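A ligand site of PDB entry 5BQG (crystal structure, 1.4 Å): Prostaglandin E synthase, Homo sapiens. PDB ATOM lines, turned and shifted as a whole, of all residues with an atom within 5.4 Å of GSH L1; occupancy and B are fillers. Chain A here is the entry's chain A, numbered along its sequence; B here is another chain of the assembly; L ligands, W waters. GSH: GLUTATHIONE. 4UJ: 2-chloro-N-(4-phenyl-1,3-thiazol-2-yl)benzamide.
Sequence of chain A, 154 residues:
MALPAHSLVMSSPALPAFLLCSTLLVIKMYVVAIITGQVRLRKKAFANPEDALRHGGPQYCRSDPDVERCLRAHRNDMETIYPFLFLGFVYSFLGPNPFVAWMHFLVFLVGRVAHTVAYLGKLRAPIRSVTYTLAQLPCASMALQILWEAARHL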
ATOM      1  N   ARG A  72      10.555  18.717  -4.101  1.00  0.00           N
ATOM      2  CA  ARG A  72      10.500  17.335  -4.618  1.00  0.00           C
ATOM      3  C   ARG A  72       9.647  17.225  -5.873  1.00  0.00           C
ATOM      4  O   ARG A  72      10.030  16.524  -6.819  1.00  0.00           O
ATOM      5  CB  ARG A  72       9.981  16.365  -3.560  1.00  0.00           C
ATOM      6  CG  ARG A  72      10.965  16.108  -2.420  1.00  0.00           C
ATOM      7  CD  ARG A  72      10.621  14.854  -1.625  1.00  0.00           C
ATOM      8  NE  ARG A  72       9.363  14.958  -0.875  1.00  0.00           N
ATOM      9  CZ  ARG A  72       9.225  15.585   0.292  1.00  0.00           C
ATOM     10  NH1 ARG A  72      10.267  16.182   0.864  1.00  0.00           N
ATOM     11  NH2 ARG A  72       8.046  15.615   0.887  1.00  0.00           N
ATOM     12  N   ALA A  73       8.507  17.902  -5.893  1.00  0.00           N
ATOM     13  CA  ALA A  73       7.657  17.927  -7.086  1.00  0.00           C
ATOM     14  C   ALA A  73       8.386  18.540  -8.267  1.00  0.00           C
ATOM     15  O   ALA A  73       8.367  17.985  -9.371  1.00  0.00           O
ATOM     16  CB  ALA A  73       6.352  18.674  -6.811  1.00  0.00           C
ATOM     17  N   ARG A  75      11.681  18.801  -8.614  1.00  0.00           N
ATOM     18  CA  ARG A  75      12.771  17.896  -8.983  1.00  0.00           C
ATOM     19  C   ARG A  75      12.264  16.733  -9.829  1.00  0.00           C
ATOM     20  O   ARG A  75      12.848  16.397 -10.864  1.00  0.00           O
ATOM     21  CB  ARG A  75      13.512  17.372  -7.740  1.00  0.00           C
ATOM     22  CG  ARG A  75      14.600  16.342  -8.059  1.00  0.00           C
ATOM     23  CD  ARG A  75      15.292  15.739  -6.838  1.00  0.00           C
ATOM     24  NE  ARG A  75      14.396  15.349  -5.743  1.00  0.00           N
ATOM     25  CZ  ARG A  75      13.488  14.367  -5.787  1.00  0.00           C
ATOM     26  NH1 ARG A  75      12.736  14.124  -4.714  1.00  0.00           N
ATOM     27  NH2 ARG A  75      13.316  13.626  -6.883  1.00  0.00           N
ATOM     28  N   ASN A  76      11.148  16.118  -9.417  1.00  0.00           N
ATOM     29  CA  ASN A  76      10.585  15.029 -10.201  1.00  0.00           C
ATOM     30  C   ASN A  76      10.182  15.484 -11.604  1.00  0.00           C
ATOM     31  O   ASN A  76      10.412  14.763 -12.577  1.00  0.00           O
ATOM     32  CB  ASN A  76       9.413  14.371  -9.444  1.00  0.00           C
ATOM     33  CG  ASN A  76       9.004  13.050 -10.061  1.00  0.00           C
ATOM     34  OD1 ASN A  76       8.229  13.016 -11.015  1.00  0.00           O
ATOM     35  ND2 ASN A  76       9.525  11.951  -9.522  1.00  0.00           N
ATOM     36  N   GLU A  79      13.252  15.486 -13.626  1.00  0.00           N
ATOM     37  CA  GLU A  79      13.629  14.106 -13.934  1.00  0.00           C
ATOM     38  C   GLU A  79      12.797  13.472 -15.055  1.00  0.00           C
ATOM     39  O   GLU A  79      13.198  12.447 -15.617  1.00  0.00           O
ATOM     40  CB  GLU A  79      13.529  13.239 -12.667  1.00  0.00           C
ATOM     41  CG  GLU A  79      14.537  13.609 -11.586  1.00  0.00           C
ATOM     42  CD  GLU A  79      14.278  12.942 -10.235  1.00  0.00           C
ATOM     43  OE1 GLU A  79      13.331  12.135 -10.119  1.00  0.00           O
ATOM     44  OE2 GLU A  79      15.044  13.238  -9.288  1.00  0.00           O
ATOM     45  N   HIS A 115       0.182  14.102 -11.528  1.00  0.00           N
ATOM     46  CA  HIS A 115       1.313  13.908 -10.609  1.00  0.00           C
ATOM     47  C   HIS A 115       1.515  15.106  -9.679  1.00  0.00           C
ATOM     48  O   HIS A 115       1.650  14.941  -8.456  1.00  0.00           O
ATOM     49  CB  HIS A 115       2.604  13.616 -11.389  1.00  0.00           C
ATOM     50  CG  HIS A 115       3.758  13.225 -10.509  1.00  0.00           C
ATOM     51  ND1 HIS A 115       4.616  14.150  -9.951  1.00  0.00           N
ATOM     52  CD2 HIS A 115       4.198  12.005 -10.114  1.00  0.00           C
ATOM     53  CE1 HIS A 115       5.530  13.517  -9.240  1.00  0.00           C
ATOM     54  NE2 HIS A 115       5.304  12.213  -9.319  1.00  0.00           N
ATOM     55  N   TYR A 119       1.004  15.175  -5.719  1.00  0.00           N
ATOM     56  CA  TYR A 119       2.152  15.469  -4.870  1.00  0.00           C
ATOM     57  C   TYR A 119       1.863  16.635  -3.934  1.00  0.00           C
ATOM     58  O   TYR A 119       1.968  16.489  -2.706  1.00  0.00           O
ATOM     59  CB  TYR A 119       3.419  15.774  -5.697  1.00  0.00           C
ATOM     60  CG  TYR A 119       4.693  15.218  -5.086  1.00  0.00           C
ATOM     61  CD1 TYR A 119       4.755  14.909  -3.727  1.00  0.00           C
ATOM     62  CD2 TYR A 119       5.831  14.993  -5.865  1.00  0.00           C
ATOM     63  CE1 TYR A 119       5.903  14.384  -3.160  1.00  0.00           C
ATOM     64  CE2 TYR A 119       6.987  14.470  -5.309  1.00  0.00           C
ATOM     65  CZ  TYR A 119       7.020  14.159  -3.947  1.00  0.00           C
ATOM     66  OH  TYR A 119       8.140  13.622  -3.359  1.00  0.00           O
ATOM     67  N   ARG A 128       0.013   9.131  -6.563  1.00  0.00           N
ATOM     68  CA  ARG A 128       1.157   9.786  -7.196  1.00  0.00           C
ATOM     69  C   ARG A 128       2.027   8.792  -7.984  1.00  0.00           C
ATOM     70  O   ARG A 128       2.420   9.073  -9.118  1.00  0.00           O
ATOM     71  CB  ARG A 128       2.005  10.540  -6.177  1.00  0.00           C
ATOM     72  CG  ARG A 128       3.071  11.425  -6.803  1.00  0.00           C
ATOM     73  CD  ARG A 128       4.130  11.844  -5.804  1.00  0.00           C
ATOM     74  NE  ARG A 128       5.026  10.738  -5.434  1.00  0.00           N
ATOM     75  CZ  ARG A 128       5.020  10.103  -4.267  1.00  0.00           C
ATOM     76  NH1 ARG A 128       4.167  10.449  -3.305  1.00  0.00           N
ATOM     77  NH2 ARG A 128       5.877   9.120  -4.054  1.00  0.00           N
ATOM     78  N   SER A 129       2.315   7.641  -7.375  1.00  0.00           N
ATOM     79  CA  SER A 129       3.140   6.613  -8.020  1.00  0.00           C
ATOM     80  C   SER A 129       2.527   6.131  -9.322  1.00  0.00           C
ATOM     81  O   SER A 129       3.241   5.934 -10.308  1.00  0.00           O
ATOM     82  CB  SER A 129       3.372   5.450  -7.064  1.00  0.00           C
ATOM     83  OG  SER A 129       4.103   5.869  -5.921  1.00  0.00           O
ATOM     84  N   TYR A 132       2.915   8.824 -12.074  1.00  0.00           N
ATOM     85  CA  TYR A 132       4.308   8.808 -12.538  1.00  0.00           C
ATOM     86  C   TYR A 132       4.528   7.677 -13.545  1.00  0.00           C
ATOM     87  O   TYR A 132       5.079   7.907 -14.629  1.00  0.00           O
ATOM     88  CB  TYR A 132       5.262   8.646 -11.356  1.00  0.00           C
ATOM     89  CG  TYR A 132       6.669   8.181 -11.729  1.00  0.00           C
ATOM     90  CD1 TYR A 132       7.615   9.082 -12.240  1.00  0.00           C
ATOM     91  CD2 TYR A 132       7.051   6.849 -11.549  1.00  0.00           C
ATOM     92  CE1 TYR A 132       8.894   8.660 -12.566  1.00  0.00           C
ATOM     93  CE2 TYR A 132       8.331   6.425 -11.864  1.00  0.00           C
ATOM     94  CZ  TYR A 132       9.248   7.326 -12.373  1.00  0.00           C
ATOM     95  OH  TYR A 132      10.528   6.902 -12.689  1.00  0.00           O
ATOM     96  N   ALA B  33      16.371   6.166 -12.077  1.00  0.00           N
ATOM     97  CA  ALA B  33      15.071   6.368 -11.425  1.00  0.00           C
ATOM     98  C   ALA B  33      14.469   5.064 -10.922  1.00  0.00           C
ATOM     99  O   ALA B  33      13.925   5.013  -9.812  1.00  0.00           O
ATOM    100  CB  ALA B  33      14.102   7.090 -12.355  1.00  0.00           C
ATOM    101  N   THR B  36      16.442   3.869  -7.883  1.00  0.00           N
ATOM    102  CA  THR B  36      16.084   4.703  -6.737  1.00  0.00           C
ATOM    103  C   THR B  36      14.810   4.180  -6.059  1.00  0.00           C
ATOM    104  O   THR B  36      14.785   4.011  -4.830  1.00  0.00           O
ATOM    105  CB  THR B  36      15.906   6.181  -7.147  1.00  0.00           C
ATOM    106  OG1 THR B  36      17.083   6.658  -7.798  1.00  0.00           O
ATOM    107  CG2 THR B  36      15.634   7.060  -5.924  1.00  0.00           C
ATOM    108  N   GLY B  37      13.776   3.915  -6.856  1.00  0.00           N
ATOM    109  CA  GLY B  37      12.507   3.387  -6.340  1.00  0.00           C
ATOM    110  C   GLY B  37      12.669   2.044  -5.645  1.00  0.00           C
ATOM    111  O   GLY B  37      12.097   1.824  -4.568  1.00  0.00           O
ATOM    112  N   ARG B  40      14.425   2.592  -2.284  1.00  0.00           N
ATOM    113  CA  ARG B  40      13.466   3.136  -1.314  1.00  0.00           C
ATOM    114  C   ARG B  40      12.618   2.036  -0.688  1.00  0.00           C
ATOM    115  O   ARG B  40      12.446   1.995   0.526  1.00  0.00           O
ATOM    116  CB  ARG B  40      12.544   4.176  -1.969  1.00  0.00           C
ATOM    117  CG  ARG B  40      13.193   5.516  -2.292  1.00  0.00           C
ATOM    118  CD  ARG B  40      12.129   6.536  -2.653  1.00  0.00           C
ATOM    119  NE  ARG B  40      12.671   7.870  -2.935  1.00  0.00           N
ATOM    120  CZ  ARG B  40      13.045   8.750  -2.000  1.00  0.00           C
ATOM    121  NH1 ARG B  40      12.970   8.443  -0.707  1.00  0.00           N
ATOM    122  NH2 ARG B  40      13.514   9.938  -2.368  1.00  0.00           N
ATOM    123  N   ALA B  47      10.188   9.460   1.000  1.00  0.00           N
ATOM    124  CA  ALA B  47      10.295  10.916   1.145  1.00  0.00           C
ATOM    125  C   ALA B  47       9.044  11.557   1.729  1.00  0.00           C
ATOM    126  O   ALA B  47       9.097  12.679   2.234  1.00  0.00           O
ATOM    127  CB  ALA B  47      10.637  11.545  -0.197  1.00  0.00           C
ATOM    128  N   ASN B  48       7.927  10.832   1.678  1.00  0.00           N
ATOM    129  CA  ASN B  48       6.614  11.384   2.008  1.00  0.00           C
ATOM    130  C   ASN B  48       5.856  10.542   3.030  1.00  0.00           C
ATOM    131  O   ASN B  48       5.868   9.315   2.944  1.00  0.00           O
ATOM    132  CB  ASN B  48       5.773  11.496   0.740  1.00  0.00           C
ATOM    133  CG  ASN B  48       6.487  12.243  -0.357  1.00  0.00           C
ATOM    134  OD1 ASN B  48       6.709  13.444  -0.255  1.00  0.00           O
ATOM    135  ND2 ASN B  48       6.860  11.522  -1.414  1.00  0.00           N
ATOM    136  N   VAL B  67      19.685   5.769  -0.782  1.00  0.00           N
ATOM    137  CA  VAL B  67      18.713   6.584  -1.512  1.00  0.00           C
ATOM    138  C   VAL B  67      19.326   7.947  -1.880  1.00  0.00           C
ATOM    139  O   VAL B  67      19.221   8.386  -3.022  1.00  0.00           O
ATOM    140  CB  VAL B  67      17.394   6.785  -0.738  1.00  0.00           C
ATOM    141  CG1 VAL B  67      16.425   7.674  -1.513  1.00  0.00           C
ATOM    142  CG2 VAL B  67      16.733   5.438  -0.444  1.00  0.00           C
ATOM    143  N   LEU B  71      19.994   9.617  -5.606  1.00  0.00           N
ATOM    144  CA  LEU B  71      19.564  10.964  -5.962  1.00  0.00           C
ATOM    145  C   LEU B  71      20.725  11.838  -6.447  1.00  0.00           C
ATOM    146  O   LEU B  71      20.548  12.638  -7.369  1.00  0.00           O
ATOM    147  CB  LEU B  71      18.810  11.637  -4.810  1.00  0.00           C
ATOM    148  CG  LEU B  71      17.408  11.096  -4.524  1.00  0.00           C
ATOM    149  CD1 LEU B  71      16.907  11.619  -3.189  1.00  0.00           C
ATOM    150  CD2 LEU B  71      16.433  11.452  -5.637  1.00  0.00           C
ATOM    151  N   HIS B  74      21.516  10.779 -10.036  1.00  0.00           N
ATOM    152  CA  HIS B  74      20.468  11.332 -10.903  1.00  0.00           C
ATOM    153  C   HIS B  74      20.643  12.838 -11.083  1.00  0.00           C
ATOM    154  O   HIS B  74      20.508  13.355 -12.195  1.00  0.00           O
ATOM    155  CB  HIS B  74      19.087  11.017 -10.328  1.00  0.00           C
ATOM    156  CG  HIS B  74      18.003  10.952 -11.364  1.00  0.00           C
ATOM    157  ND1 HIS B  74      16.790  10.329 -11.125  1.00  0.00           N
ATOM    158  CD2 HIS B  74      17.945  11.405 -12.641  1.00  0.00           C
ATOM    159  CE1 HIS B  74      16.029  10.416 -12.201  1.00  0.00           C
ATOM    160  NE2 HIS B  74      16.711  11.058 -13.142  1.00  0.00           N
HETATM  161  N1  GSH L   1      13.866  10.551  -7.838  1.00  0.00           N
HETATM  162  CA1 GSH L   1      12.685   9.654  -7.675  1.00  0.00           C
HETATM  163  C1  GSH L   1      12.465   9.301  -6.231  1.00  0.00           C
HETATM  164  O11 GSH L   1      11.422   8.684  -5.898  1.00  0.00           O
HETATM  165  O12 GSH L   1      13.320   9.648  -5.389  1.00  0.00           O
HETATM  166  CB1 GSH L   1      12.889   8.423  -8.568  1.00  0.00           C
HETATM  167  CG1 GSH L   1      11.667   7.514  -8.726  1.00  0.00           C
HETATM  168  CD1 GSH L   1      10.380   8.280  -8.995  1.00  0.00           C
HETATM  169  OE1 GSH L   1      10.352   9.184  -9.802  1.00  0.00           O
HETATM  170  N2  GSH L   1       9.315   7.900  -8.286  1.00  0.00           N
HETATM  171  CA2 GSH L   1       8.016   8.542  -8.403  1.00  0.00           C
HETATM  172  C2  GSH L   1       7.878   9.778  -7.547  1.00  0.00           C
HETATM  173  O2  GSH L   1       6.853  10.454  -7.628  1.00  0.00           O
HETATM  174  CB2 GSH L   1       6.896   7.550  -8.053  1.00  0.00           C
HETATM  175  SG2 GSH L   1       6.981   6.911  -6.362  1.00  0.00           S
HETATM  176  N3  GSH L   1       8.893  10.072  -6.725  1.00  0.00           N
HETATM  177  CA3 GSH L   1       8.842  11.149  -5.750  1.00  0.00           C
HETATM  178  C3  GSH L   1       9.987  12.130  -5.851  1.00  0.00           C
HETATM  179  O31 GSH L   1      10.777  12.085  -6.832  1.00  0.00           O
HETATM  180  O32 GSH L   1      10.109  12.975  -4.933  1.00  0.00           O
HETATM  181  C7  4UJ L   2       8.399   4.927  -3.305  1.00  0.00           C
HETATM  182  C6  4UJ L   2       7.171   5.381  -2.861  1.00  0.00           C
HETATM  183  C1  4UJ L   2       1.514   0.644  -6.595  1.00  0.00           C
HETATM  184  N1  4UJ L   2       4.651   2.504  -5.650  1.00  0.00           N
HETATM  185  C5  4UJ L   2       6.017   4.668  -3.180  1.00  0.00           C
HETATM  186  C4  4UJ L   2       6.080   3.513  -3.951  1.00  0.00           C
HETATM  187  C3  4UJ L   2       4.856   2.721  -4.300  1.00  0.00           C
HETATM  188  C2  4UJ L   2       3.537   1.869  -6.158  1.00  0.00           C
HETATM  189 CL   4UJ L   2       4.496   5.263  -2.603  1.00  0.00          CL
HETATM  190  C8  4UJ L   2       8.484   3.781  -4.058  1.00  0.00           C
HETATM  191  C9  4UJ L   2       7.330   3.068  -4.377  1.00  0.00           C
HETATM  192  O   4UJ L   2       4.099   2.305  -3.433  1.00  0.00           O
HETATM  193  S   4UJ L   2       2.394   1.021  -5.168  1.00  0.00           S
HETATM  194  N   4UJ L   2       3.291   1.866  -7.445  1.00  0.00           N
HETATM  195  C   4UJ L   2       2.113   1.148  -7.701  1.00  0.00           C
HETATM  196  C10 4UJ L   2       1.631   1.008  -9.087  1.00  0.00           C
HETATM  197  C15 4UJ L   2       0.676   0.050  -9.417  1.00  0.00           C
HETATM  198  C14 4UJ L   2       0.212  -0.088 -10.714  1.00  0.00           C
HETATM  199  C13 4UJ L   2       0.711   0.745 -11.711  1.00  0.00           C
HETATM  200  C12 4UJ L   2       1.655   1.695 -11.401  1.00  0.00           C
HETATM  201  C11 4UJ L   2       2.119   1.832 -10.104  1.00  0.00           C
HETATM  202  O   HOH W   1       9.370   7.980  -4.179  1.00  0.00           O
HETATM  203  O   HOH W   2      16.259   9.336  -8.555  1.00  0.00           O
HETATM  204  O   HOH W   3       9.579   5.144  -6.915  1.00  0.00           O
HETATM  205  O   HOH W   4      12.128  10.223 -11.757  1.00  0.00           O
HETATM  206  O   HOH W   5       6.450   3.960  -7.440  1.00  0.00           O
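OH of Tyr 119 sits at hydrogen-bond distance from O32 of GSH L1 (2.6 Å).
The side-chain carboxylate (OE1) of Glu 79 lies within salt-bridge range of a nitrogen (N1) of GSH L1, 2.8 Å away.
O2 of GSH L1 is in hydrogen-bond range of NE of Arg 128 (2.9 Å).
OG of Ser 129 sits close to SG2 of GSH L1 (3.1 Å).
NH1 of Arg 75 lies within salt-bridge range of O32 of GSH L1 (2.9 Å).
The side-chain hydroxyl (OG) of Ser 129 is in hydrogen-bond range of a nitrogen (N1) of 4UJ L2, 3.4 Å away.
An oxygen (OE1) of GSH L1 lies within hydrogen-bond range of the side-chain amide nitrogen of Asn 76 (2.9 Å).
NH2 of Arg 40 of chain B is in salt-bridge range of O12 of GSH L1.
A ring nitrogen (NE2) of His 115 lies within hydrogen-bond range of an oxygen (O2) of GSH L1 (2.9 Å).
ND2 of Asn 48 of chain B lies close to NH1 of Arg 128, 3.5 Å away.
The side-chain hydroxyl of Tyr 119 is in hydrogen-bond range of the guanidinium group of Arg 72 (3.1 Å).
The side-chain hydroxyl (OH) of Tyr 119 is in hydrogen-bond range of the side-chain amide nitrogen (ND2) of Asn 48 of chain B (3.1 Å).
O of Ala 47 of chain B lies within hydrogen-bond range of NH2 of Arg 72.
The side-chain amide oxygen (OD1) of Asn 48 of chain B lies within hydrogen-bond range of the guanidinium group (NH2) of Arg 72.
OE2 of Glu 79 is in salt-bridge range of NH2 of Arg 75.
A ring nitrogen (NE2) of His 115 lies close to the side-chain amide oxygen (OD1) of Asn 76, 3.5 Å away.
Arg 72 touches GSH L1 (CB to O32, 3.7 Å).
CE1 of Tyr 132 touches OE1 of GSH L1, at 3.2 Å.
Ala 33 of chain B touches GSH L1 (O to CG1, 3.5 Å).
Thr 36 of chain B touches GSH L1.
CD2 of Leu 71 of chain B touches N1 of GSH L1 (3.5 Å).
Within 4 Å of GSH L1: Arg 72, Arg 75, Asn 76, Glu 79, His 115, Tyr 119, Arg 128, Ser 129, Tyr 132, Ala 33 of chain B, Thr 36 of chain B, Arg 40 of chain B and Leu 71 of chain B.
Along chain A the residues within 4 Å of GSH L1 span positions 72 to 132.
Water W2 lies within hydrogen-bond range of a nitrogen (N1) of GSH L1, a ring nitrogen (ND1) of His 74 of chain B and the side-chain hydroxyl of Thr 36 of chain B.
Water W4 bridges OE1 of Glu 79 and OE1 of GSH L1.
Water W5 lies within hydrogen-bond range of N1 of 4UJ L2 (2.9 Å), SG2 of GSH L1 (3.2 Å) and OG of Ser 129 (3.4 Å).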
